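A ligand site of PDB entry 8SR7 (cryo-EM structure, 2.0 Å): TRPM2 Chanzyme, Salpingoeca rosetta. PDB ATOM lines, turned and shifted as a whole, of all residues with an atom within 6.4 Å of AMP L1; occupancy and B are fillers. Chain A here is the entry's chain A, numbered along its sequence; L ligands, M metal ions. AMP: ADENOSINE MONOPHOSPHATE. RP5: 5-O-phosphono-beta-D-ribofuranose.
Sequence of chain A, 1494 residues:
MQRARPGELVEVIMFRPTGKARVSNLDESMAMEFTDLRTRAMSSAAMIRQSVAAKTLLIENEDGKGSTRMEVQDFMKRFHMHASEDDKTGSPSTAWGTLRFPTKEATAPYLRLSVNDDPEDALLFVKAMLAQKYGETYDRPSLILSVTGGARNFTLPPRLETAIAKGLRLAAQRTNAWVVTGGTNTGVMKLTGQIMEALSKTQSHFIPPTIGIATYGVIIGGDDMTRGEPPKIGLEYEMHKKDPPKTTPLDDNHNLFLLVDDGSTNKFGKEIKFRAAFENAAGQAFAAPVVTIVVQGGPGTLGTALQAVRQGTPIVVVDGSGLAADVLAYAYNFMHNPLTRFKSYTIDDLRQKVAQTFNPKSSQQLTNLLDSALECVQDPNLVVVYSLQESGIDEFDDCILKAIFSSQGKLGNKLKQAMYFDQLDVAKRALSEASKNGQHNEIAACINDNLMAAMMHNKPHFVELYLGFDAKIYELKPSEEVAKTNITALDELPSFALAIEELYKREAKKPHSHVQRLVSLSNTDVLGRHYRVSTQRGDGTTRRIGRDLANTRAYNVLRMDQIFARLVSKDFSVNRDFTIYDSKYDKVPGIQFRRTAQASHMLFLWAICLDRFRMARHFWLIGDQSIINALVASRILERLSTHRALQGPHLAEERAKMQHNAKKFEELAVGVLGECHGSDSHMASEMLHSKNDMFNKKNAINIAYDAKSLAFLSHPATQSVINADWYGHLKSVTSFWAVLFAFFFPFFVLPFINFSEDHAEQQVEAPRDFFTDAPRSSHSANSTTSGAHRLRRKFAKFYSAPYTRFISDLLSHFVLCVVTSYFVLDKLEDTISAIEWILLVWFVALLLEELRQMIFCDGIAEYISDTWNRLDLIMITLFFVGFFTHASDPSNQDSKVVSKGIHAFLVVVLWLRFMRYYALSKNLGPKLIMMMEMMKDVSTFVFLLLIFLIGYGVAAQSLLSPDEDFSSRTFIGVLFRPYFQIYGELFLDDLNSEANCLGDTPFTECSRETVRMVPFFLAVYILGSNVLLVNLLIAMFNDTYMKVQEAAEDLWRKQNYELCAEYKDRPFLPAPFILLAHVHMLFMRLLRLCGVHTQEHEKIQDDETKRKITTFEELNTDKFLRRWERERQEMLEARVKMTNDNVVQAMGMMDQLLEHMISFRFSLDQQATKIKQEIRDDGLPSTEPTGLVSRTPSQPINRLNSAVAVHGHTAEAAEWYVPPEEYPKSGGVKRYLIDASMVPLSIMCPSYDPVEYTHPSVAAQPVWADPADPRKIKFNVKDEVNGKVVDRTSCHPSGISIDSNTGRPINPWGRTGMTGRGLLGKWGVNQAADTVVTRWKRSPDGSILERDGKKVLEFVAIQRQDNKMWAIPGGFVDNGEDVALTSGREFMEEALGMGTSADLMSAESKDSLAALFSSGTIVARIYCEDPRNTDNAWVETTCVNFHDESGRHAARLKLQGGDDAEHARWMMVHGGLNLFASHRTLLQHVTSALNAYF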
ATOM      1  N   VAL A1258      10.068 -22.115 -24.550  1.00  0.00           N
ATOM      2  CA  VAL A1258      10.305 -23.349 -25.299  1.00  0.00           C
ATOM      3  C   VAL A1258      10.588 -23.045 -26.776  1.00  0.00           C
ATOM      4  O   VAL A1258      11.535 -23.583 -27.362  1.00  0.00           O
ATOM      5  CB  VAL A1258       9.096 -24.284 -25.093  1.00  0.00           C
ATOM      6  CG1 VAL A1258       9.055 -25.460 -26.084  1.00  0.00           C
ATOM      7  CG2 VAL A1258       9.080 -24.810 -23.672  1.00  0.00           C
ATOM      8  N   TRP A1264      17.721 -27.910 -23.691  1.00  0.00           N
ATOM      9  CA  TRP A1264      16.876 -29.009 -23.229  1.00  0.00           C
ATOM     10  C   TRP A1264      15.597 -29.141 -24.039  1.00  0.00           C
ATOM     11  O   TRP A1264      14.708 -29.909 -23.654  1.00  0.00           O
ATOM     12  CB  TRP A1264      16.515 -28.826 -21.744  1.00  0.00           C
ATOM     13  CG  TRP A1264      16.143 -27.439 -21.331  1.00  0.00           C
ATOM     14  CD1 TRP A1264      16.987 -26.482 -20.829  1.00  0.00           C
ATOM     15  CD2 TRP A1264      14.847 -26.833 -21.392  1.00  0.00           C
ATOM     16  NE1 TRP A1264      16.284 -25.325 -20.561  1.00  0.00           N
ATOM     17  CE2 TRP A1264      14.971 -25.514 -20.897  1.00  0.00           C
ATOM     18  CE3 TRP A1264      13.583 -27.280 -21.815  1.00  0.00           C
ATOM     19  CZ2 TRP A1264      13.881 -24.639 -20.815  1.00  0.00           C
ATOM     20  CZ3 TRP A1264      12.494 -26.415 -21.727  1.00  0.00           C
ATOM     21  CH2 TRP A1264      12.659 -25.099 -21.230  1.00  0.00           C
ATOM     22  N   ALA A1265      15.470 -28.401 -25.135  1.00  0.00           N
ATOM     23  CA  ALA A1265      14.275 -28.406 -25.966  1.00  0.00           C
ATOM     24  C   ALA A1265      14.512 -29.161 -27.270  1.00  0.00           C
ATOM     25  O   ALA A1265      15.539 -28.971 -27.930  1.00  0.00           O
ATOM     26  CB  ALA A1265      13.827 -26.979 -26.282  1.00  0.00           C
ATOM     27  N   LEU A1319       4.656 -25.665 -22.045  1.00  0.00           N
ATOM     28  CA  LEU A1319       5.845 -25.369 -21.247  1.00  0.00           C
ATOM     29  C   LEU A1319       6.876 -26.483 -21.269  1.00  0.00           C
ATOM     30  O   LEU A1319       7.975 -26.296 -20.732  1.00  0.00           O
ATOM     31  CB  LEU A1319       5.471 -25.090 -19.791  1.00  0.00           C
ATOM     32  CG  LEU A1319       5.118 -23.681 -19.344  1.00  0.00           C
ATOM     33  CD1 LEU A1319       4.459 -23.751 -17.990  1.00  0.00           C
ATOM     34  CD2 LEU A1319       6.372 -22.849 -19.266  1.00  0.00           C
ATOM     35  N   LEU A1320       6.546 -27.632 -21.838  1.00  0.00           N
ATOM     36  CA  LEU A1320       7.431 -28.781 -21.845  1.00  0.00           C
ATOM     37  C   LEU A1320       8.344 -28.757 -23.054  1.00  0.00           C
ATOM     38  O   LEU A1320       7.909 -28.475 -24.171  1.00  0.00           O
ATOM     39  CB  LEU A1320       6.587 -30.051 -21.825  1.00  0.00           C
ATOM     40  CG  LEU A1320       5.677 -30.170 -20.598  1.00  0.00           C
ATOM     41  CD1 LEU A1320       4.902 -31.457 -20.670  1.00  0.00           C
ATOM     42  CD2 LEU A1320       6.440 -30.085 -19.274  1.00  0.00           C
ATOM     43  N   GLY A1321       9.622 -29.072 -22.833  1.00  0.00           N
ATOM     44  CA  GLY A1321      10.604 -28.903 -23.880  1.00  0.00           C
ATOM     45  C   GLY A1321      10.743 -30.061 -24.843  1.00  0.00           C
ATOM     46  O   GLY A1321      11.196 -29.873 -25.969  1.00  0.00           O
ATOM     47  N   LYS A1322      10.331 -31.261 -24.430  1.00  0.00           N
ATOM     48  CA  LYS A1322      10.541 -32.451 -25.238  1.00  0.00           C
ATOM     49  C   LYS A1322       9.204 -32.985 -25.718  1.00  0.00           C
ATOM     50  O   LYS A1322       8.227 -32.972 -24.950  1.00  0.00           O
ATOM     51  CB  LYS A1322      11.262 -33.541 -24.439  1.00  0.00           C
ATOM     52  CG  LYS A1322      12.619 -33.156 -23.923  1.00  0.00           C
ATOM     53  CD  LYS A1322      13.281 -34.278 -23.165  1.00  0.00           C
ATOM     54  CE  LYS A1322      14.464 -33.766 -22.370  1.00  0.00           C
ATOM     55  NZ  LYS A1322      15.405 -33.029 -23.248  1.00  0.00           N
ATOM     56  N   ASN A1326       8.243 -36.524 -21.210  1.00  0.00           N
ATOM     57  CA  ASN A1326       9.216 -35.781 -20.419  1.00  0.00           C
ATOM     58  C   ASN A1326       9.471 -36.612 -19.167  1.00  0.00           C
ATOM     59  O   ASN A1326       8.588 -36.762 -18.322  1.00  0.00           O
ATOM     60  CB  ASN A1326       8.662 -34.409 -20.070  1.00  0.00           C
ATOM     61  CG  ASN A1326       8.738 -33.448 -21.214  1.00  0.00           C
ATOM     62  OD1 ASN A1326       9.787 -32.882 -21.485  1.00  0.00           O
ATOM     63  ND2 ASN A1326       7.654 -33.333 -21.959  1.00  0.00           N
ATOM     64  N   GLN A1327      10.673 -37.184 -19.082  1.00  0.00           N
ATOM     65  CA  GLN A1327      11.007 -38.041 -17.962  1.00  0.00           C
ATOM     66  C   GLN A1327      11.376 -37.171 -16.776  1.00  0.00           C
ATOM     67  O   GLN A1327      12.313 -36.360 -16.864  1.00  0.00           O
ATOM     68  CB  GLN A1327      12.154 -38.990 -18.322  1.00  0.00           C
ATOM     69  CG  GLN A1327      11.965 -39.796 -19.607  1.00  0.00           C
ATOM     70  CD  GLN A1327      11.060 -41.025 -19.475  1.00  0.00           C
ATOM     71  OE1 GLN A1327      10.574 -41.367 -18.391  1.00  0.00           O
ATOM     72  NE2 GLN A1327      10.864 -41.715 -20.584  1.00  0.00           N
ATOM     73  N   ARG A1360       7.089 -24.932  -4.046  1.00  0.00           N
ATOM     74  CA  ARG A1360       7.438 -24.557  -5.412  1.00  0.00           C
ATOM     75  C   ARG A1360       7.378 -23.058  -5.656  1.00  0.00           C
ATOM     76  O   ARG A1360       6.561 -22.345  -5.059  1.00  0.00           O
ATOM     77  CB  ARG A1360       6.535 -25.275  -6.409  1.00  0.00           C
ATOM     78  CG  ARG A1360       6.599 -26.770  -6.304  1.00  0.00           C
ATOM     79  CD  ARG A1360       5.692 -27.390  -7.330  1.00  0.00           C
ATOM     80  NE  ARG A1360       5.945 -26.878  -8.671  1.00  0.00           N
ATOM     81  CZ  ARG A1360       6.835 -27.372  -9.520  1.00  0.00           C
ATOM     82  NH1 ARG A1360       7.608 -28.390  -9.192  1.00  0.00           N
ATOM     83  NH2 ARG A1360       6.969 -26.825 -10.723  1.00  0.00           N
ATOM     84  N   ASP A1362       6.786 -21.559  -8.629  1.00  0.00           N
ATOM     85  CA  ASP A1362       5.814 -21.141  -9.650  1.00  0.00           C
ATOM     86  C   ASP A1362       4.368 -21.086  -9.143  1.00  0.00           C
ATOM     87  O   ASP A1362       3.653 -20.118  -9.432  1.00  0.00           O
ATOM     88  CB  ASP A1362       5.996 -22.005 -10.907  1.00  0.00           C
ATOM     89  CG  ASP A1362       5.795 -23.519 -10.684  1.00  0.00           C
ATOM     90  OD1 ASP A1362       5.578 -23.989  -9.548  1.00  0.00           O
ATOM     91  OD2 ASP A1362       5.860 -24.255 -11.694  1.00  0.00           O
ATOM     92  N   GLY A1371      12.877 -33.229 -10.688  1.00  0.00           N
ATOM     93  CA  GLY A1371      12.971 -32.439 -11.898  1.00  0.00           C
ATOM     94  C   GLY A1371      13.156 -33.319 -13.100  1.00  0.00           C
ATOM     95  O   GLY A1371      13.220 -34.551 -12.978  1.00  0.00           O
ATOM     96  N   PHE A1372      13.140 -32.681 -14.265  1.00  0.00           N
ATOM     97  CA  PHE A1372      13.246 -33.352 -15.548  1.00  0.00           C
ATOM     98  C   PHE A1372      14.621 -33.957 -15.759  1.00  0.00           C
ATOM     99  O   PHE A1372      15.641 -33.404 -15.330  1.00  0.00           O
ATOM    100  CB  PHE A1372      12.919 -32.381 -16.672  1.00  0.00           C
ATOM    101  CG  PHE A1372      11.502 -31.909 -16.651  1.00  0.00           C
ATOM    102  CD1 PHE A1372      10.470 -32.773 -17.037  1.00  0.00           C
ATOM    103  CD2 PHE A1372      11.203 -30.611 -16.211  1.00  0.00           C
ATOM    104  CE1 PHE A1372       9.139 -32.344 -17.014  1.00  0.00           C
ATOM    105  CE2 PHE A1372       9.871 -30.169 -16.162  1.00  0.00           C
ATOM    106  CZ  PHE A1372       8.839 -31.038 -16.579  1.00  0.00           C
ATOM    107  N   VAL A1373      14.647 -35.145 -16.389  1.00  0.00           N
ATOM    108  CA  VAL A1373      15.887 -35.837 -16.681  1.00  0.00           C
ATOM    109  C   VAL A1373      16.601 -35.150 -17.844  1.00  0.00           C
ATOM    110  O   VAL A1373      16.017 -34.962 -18.925  1.00  0.00           O
ATOM    111  CB  VAL A1373      15.610 -37.322 -16.976  1.00  0.00           C
ATOM    112  CG1 VAL A1373      16.795 -38.023 -17.651  1.00  0.00           C
ATOM    113  CG2 VAL A1373      15.229 -38.046 -15.695  1.00  0.00           C
ATOM    114  N   ASP A1374      17.839 -34.712 -17.599  1.00  0.00           N
ATOM    115  CA  ASP A1374      18.650 -34.021 -18.591  1.00  0.00           C
ATOM    116  C   ASP A1374      19.146 -35.003 -19.664  1.00  0.00           C
ATOM    117  O   ASP A1374      19.069 -36.225 -19.505  1.00  0.00           O
ATOM    118  CB  ASP A1374      19.836 -33.332 -17.914  1.00  0.00           C
ATOM    119  CG  ASP A1374      19.478 -31.992 -17.316  1.00  0.00           C
ATOM    120  OD1 ASP A1374      18.401 -31.458 -17.652  1.00  0.00           O
ATOM    121  OD2 ASP A1374      20.267 -31.469 -16.501  1.00  0.00           O
ATOM    122  N   ARG A1428       0.699 -28.729 -16.735  1.00  0.00           N
ATOM    123  CA  ARG A1428       1.407 -28.347 -17.949  1.00  0.00           C
ATOM    124  C   ARG A1428       1.344 -29.389 -19.047  1.00  0.00           C
ATOM    125  O   ARG A1428       1.946 -29.154 -20.104  1.00  0.00           O
ATOM    126  CB  ARG A1428       2.878 -28.058 -17.641  1.00  0.00           C
ATOM    127  CG  ARG A1428       3.115 -27.049 -16.544  1.00  0.00           C
ATOM    128  CD  ARG A1428       4.547 -27.129 -16.059  1.00  0.00           C
ATOM    129  NE  ARG A1428       4.787 -28.333 -15.278  1.00  0.00           N
ATOM    130  CZ  ARG A1428       5.937 -28.630 -14.694  1.00  0.00           C
ATOM    131  NH1 ARG A1428       6.986 -27.833 -14.794  1.00  0.00           N
ATOM    132  NH2 ARG A1428       6.043 -29.758 -13.990  1.00  0.00           N
ATOM    133  N   ASP A1460      14.613 -23.478  -7.611  1.00  0.00           N
ATOM    134  CA  ASP A1460      13.169 -23.307  -7.905  1.00  0.00           C
ATOM    135  C   ASP A1460      12.356 -23.844  -6.735  1.00  0.00           C
ATOM    136  O   ASP A1460      11.409 -24.598  -6.963  1.00  0.00           O
ATOM    137  CB  ASP A1460      12.813 -24.000  -9.210  1.00  0.00           C
ATOM    138  CG  ASP A1460      13.073 -25.493  -9.239  1.00  0.00           C
ATOM    139  OD1 ASP A1460      14.176 -25.896  -8.860  1.00  0.00           O
ATOM    140  OD2 ASP A1460      12.168 -26.242  -9.638  1.00  0.00           O
HETATM  141  P   AMP L   1      10.280 -24.934 -13.503  1.00  0.00           P
HETATM  142  O1P AMP L   1       9.886 -25.440 -12.135  1.00  0.00           O
HETATM  143  O2P AMP L   1       9.090 -24.464 -14.307  1.00  0.00           O
HETATM  144  O3P AMP L   1      11.387 -23.886 -13.431  1.00  0.00           O
HETATM  145  O5' AMP L   1      10.900 -26.181 -14.316  1.00  0.00           O
HETATM  146  C5' AMP L   1      12.240 -26.643 -14.002  1.00  0.00           C
HETATM  147  C4' AMP L   1      13.185 -26.270 -15.127  1.00  0.00           C
HETATM  148  O4' AMP L   1      13.706 -27.469 -15.740  1.00  0.00           O
HETATM  149  C3' AMP L   1      12.569 -25.525 -16.316  1.00  0.00           C
HETATM  150  O3' AMP L   1      12.463 -24.133 -16.048  1.00  0.00           O
HETATM  151  C2' AMP L   1      13.612 -25.788 -17.413  1.00  0.00           C
HETATM  152  O2' AMP L   1      14.625 -24.816 -17.393  1.00  0.00           O
HETATM  153  C1' AMP L   1      14.187 -27.148 -17.029  1.00  0.00           C
HETATM  154  N9  AMP L   1      13.866 -28.239 -17.936  1.00  0.00           N
HETATM  155  C8  AMP L   1      14.734 -29.222 -18.328  1.00  0.00           C
HETATM  156  N7  AMP L   1      14.200 -30.097 -19.141  1.00  0.00           N
HETATM  157  C5  AMP L   1      12.893 -29.675 -19.284  1.00  0.00           C
HETATM  158  C6  AMP L   1      11.815 -30.195 -20.016  1.00  0.00           C
HETATM  159  N6  AMP L   1      11.895 -31.290 -20.764  1.00  0.00           N
HETATM  160  N1  AMP L   1      10.639 -29.539 -19.954  1.00  0.00           N
HETATM  161  C2  AMP L   1      10.559 -28.439 -19.197  1.00  0.00           C
HETATM  162  N3  AMP L   1      11.508 -27.858 -18.467  1.00  0.00           N
HETATM  163  C4  AMP L   1      12.665 -28.526 -18.546  1.00  0.00           C
HETATM  164  C1  RP5 L   2       5.859 -33.292 -11.810  1.00  0.00           C
HETATM  165  O4  RP5 L   2       6.609 -32.104 -12.357  1.00  0.00           O
HETATM  166  C2  RP5 L   2       7.035 -34.245 -11.280  1.00  0.00           C
HETATM  167  O2  RP5 L   2       6.555 -35.010 -10.070  1.00  0.00           O
HETATM  168  C3  RP5 L   2       7.996 -33.507 -11.021  1.00  0.00           C
HETATM  169  O3  RP5 L   2       8.297 -33.479  -9.574  1.00  0.00           O
HETATM  170  C4  RP5 L   2       7.587 -31.967 -11.522  1.00  0.00           C
HETATM  171  C5  RP5 L   2       8.749 -31.309 -12.181  1.00  0.00           C
HETATM  172  O5  RP5 L   2       9.312 -30.397 -11.286  1.00  0.00           O
HETATM  173  P'  RP5 L   2      10.107 -29.107 -11.910  1.00  0.00           P
HETATM  174  O1X RP5 L   2      11.008 -28.509 -10.860  1.00  0.00           O
HETATM  175  O2X RP5 L   2       9.117 -28.084 -12.383  1.00  0.00           O
HETATM  176  O3X RP5 L   2      10.942 -29.586 -13.076  1.00  0.00           O
HETATM  177  O1  RP5 L   2       5.203 -33.865 -12.732  1.00  0.00           O
HETATM  178 MG    MG M   1      13.672 -28.832 -12.878  1.00  0.00          MG
HETATM  179 MG    MG M   2      12.092 -29.193  -9.158  1.00  0.00          MG
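The side-chain amide oxygen of Asn 1326 is in hydrogen-bond range of a nitrogen (N6) of AMP L1 (2.7 Å). N1 of AMP L1 lies within hydrogen-bond range of N of Gly 1321, at 3.1 Å. NH2 of Arg 1360 is in salt-bridge range of O1P of AMP L1 (3.5 Å). An oxygen (O2X) of RP5 L2 lies within salt-bridge range of the guanidinium group of Arg 1360 (3.0 Å). NH1 of Arg 1428 lies within salt-bridge range of O2X of RP5 L2.
An oxygen (O1P) of AMP L1 lies close to an oxygen (O2X) of RP5 L2 (2.8 Å).
The backbone carbonyl oxygen (O) of Lys 1322 sits at hydrogen-bond distance from the side-chain amide nitrogen (ND2) of Asn 1326 (3.1 Å). The side-chain amino group (NZ) of Lys 1322 is in hydrogen-bond range of the backbone carbonyl oxygen (O) of Trp 1264, at 3.2 Å. The guanidinium group (NH2) of Arg 1360 lies within salt-bridge range of the side-chain carboxylate (OD2) of Asp 1362 (3.0 Å).
O1P of AMP L1 sits close to OD2 of Asp 1460 (3.5 Å). Merely in contact with AMP L1: Phe 1372, Trp 1264, Leu 1319, Lys 1322 and Leu 1320. Hydrophobic or aromatic side chains that line AMP L1: Trp 1264 and Phe 1372. Within 4 Å of AMP L1: Trp 1264, Leu 1319, Leu 1320, Gly 1321, Lys 1322, Asn 1326, Arg 1360, Phe 1372 and Asp 1460. The nearest printed residue that does not touch AMP L1 is Arg 1428 (4.002 Å).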
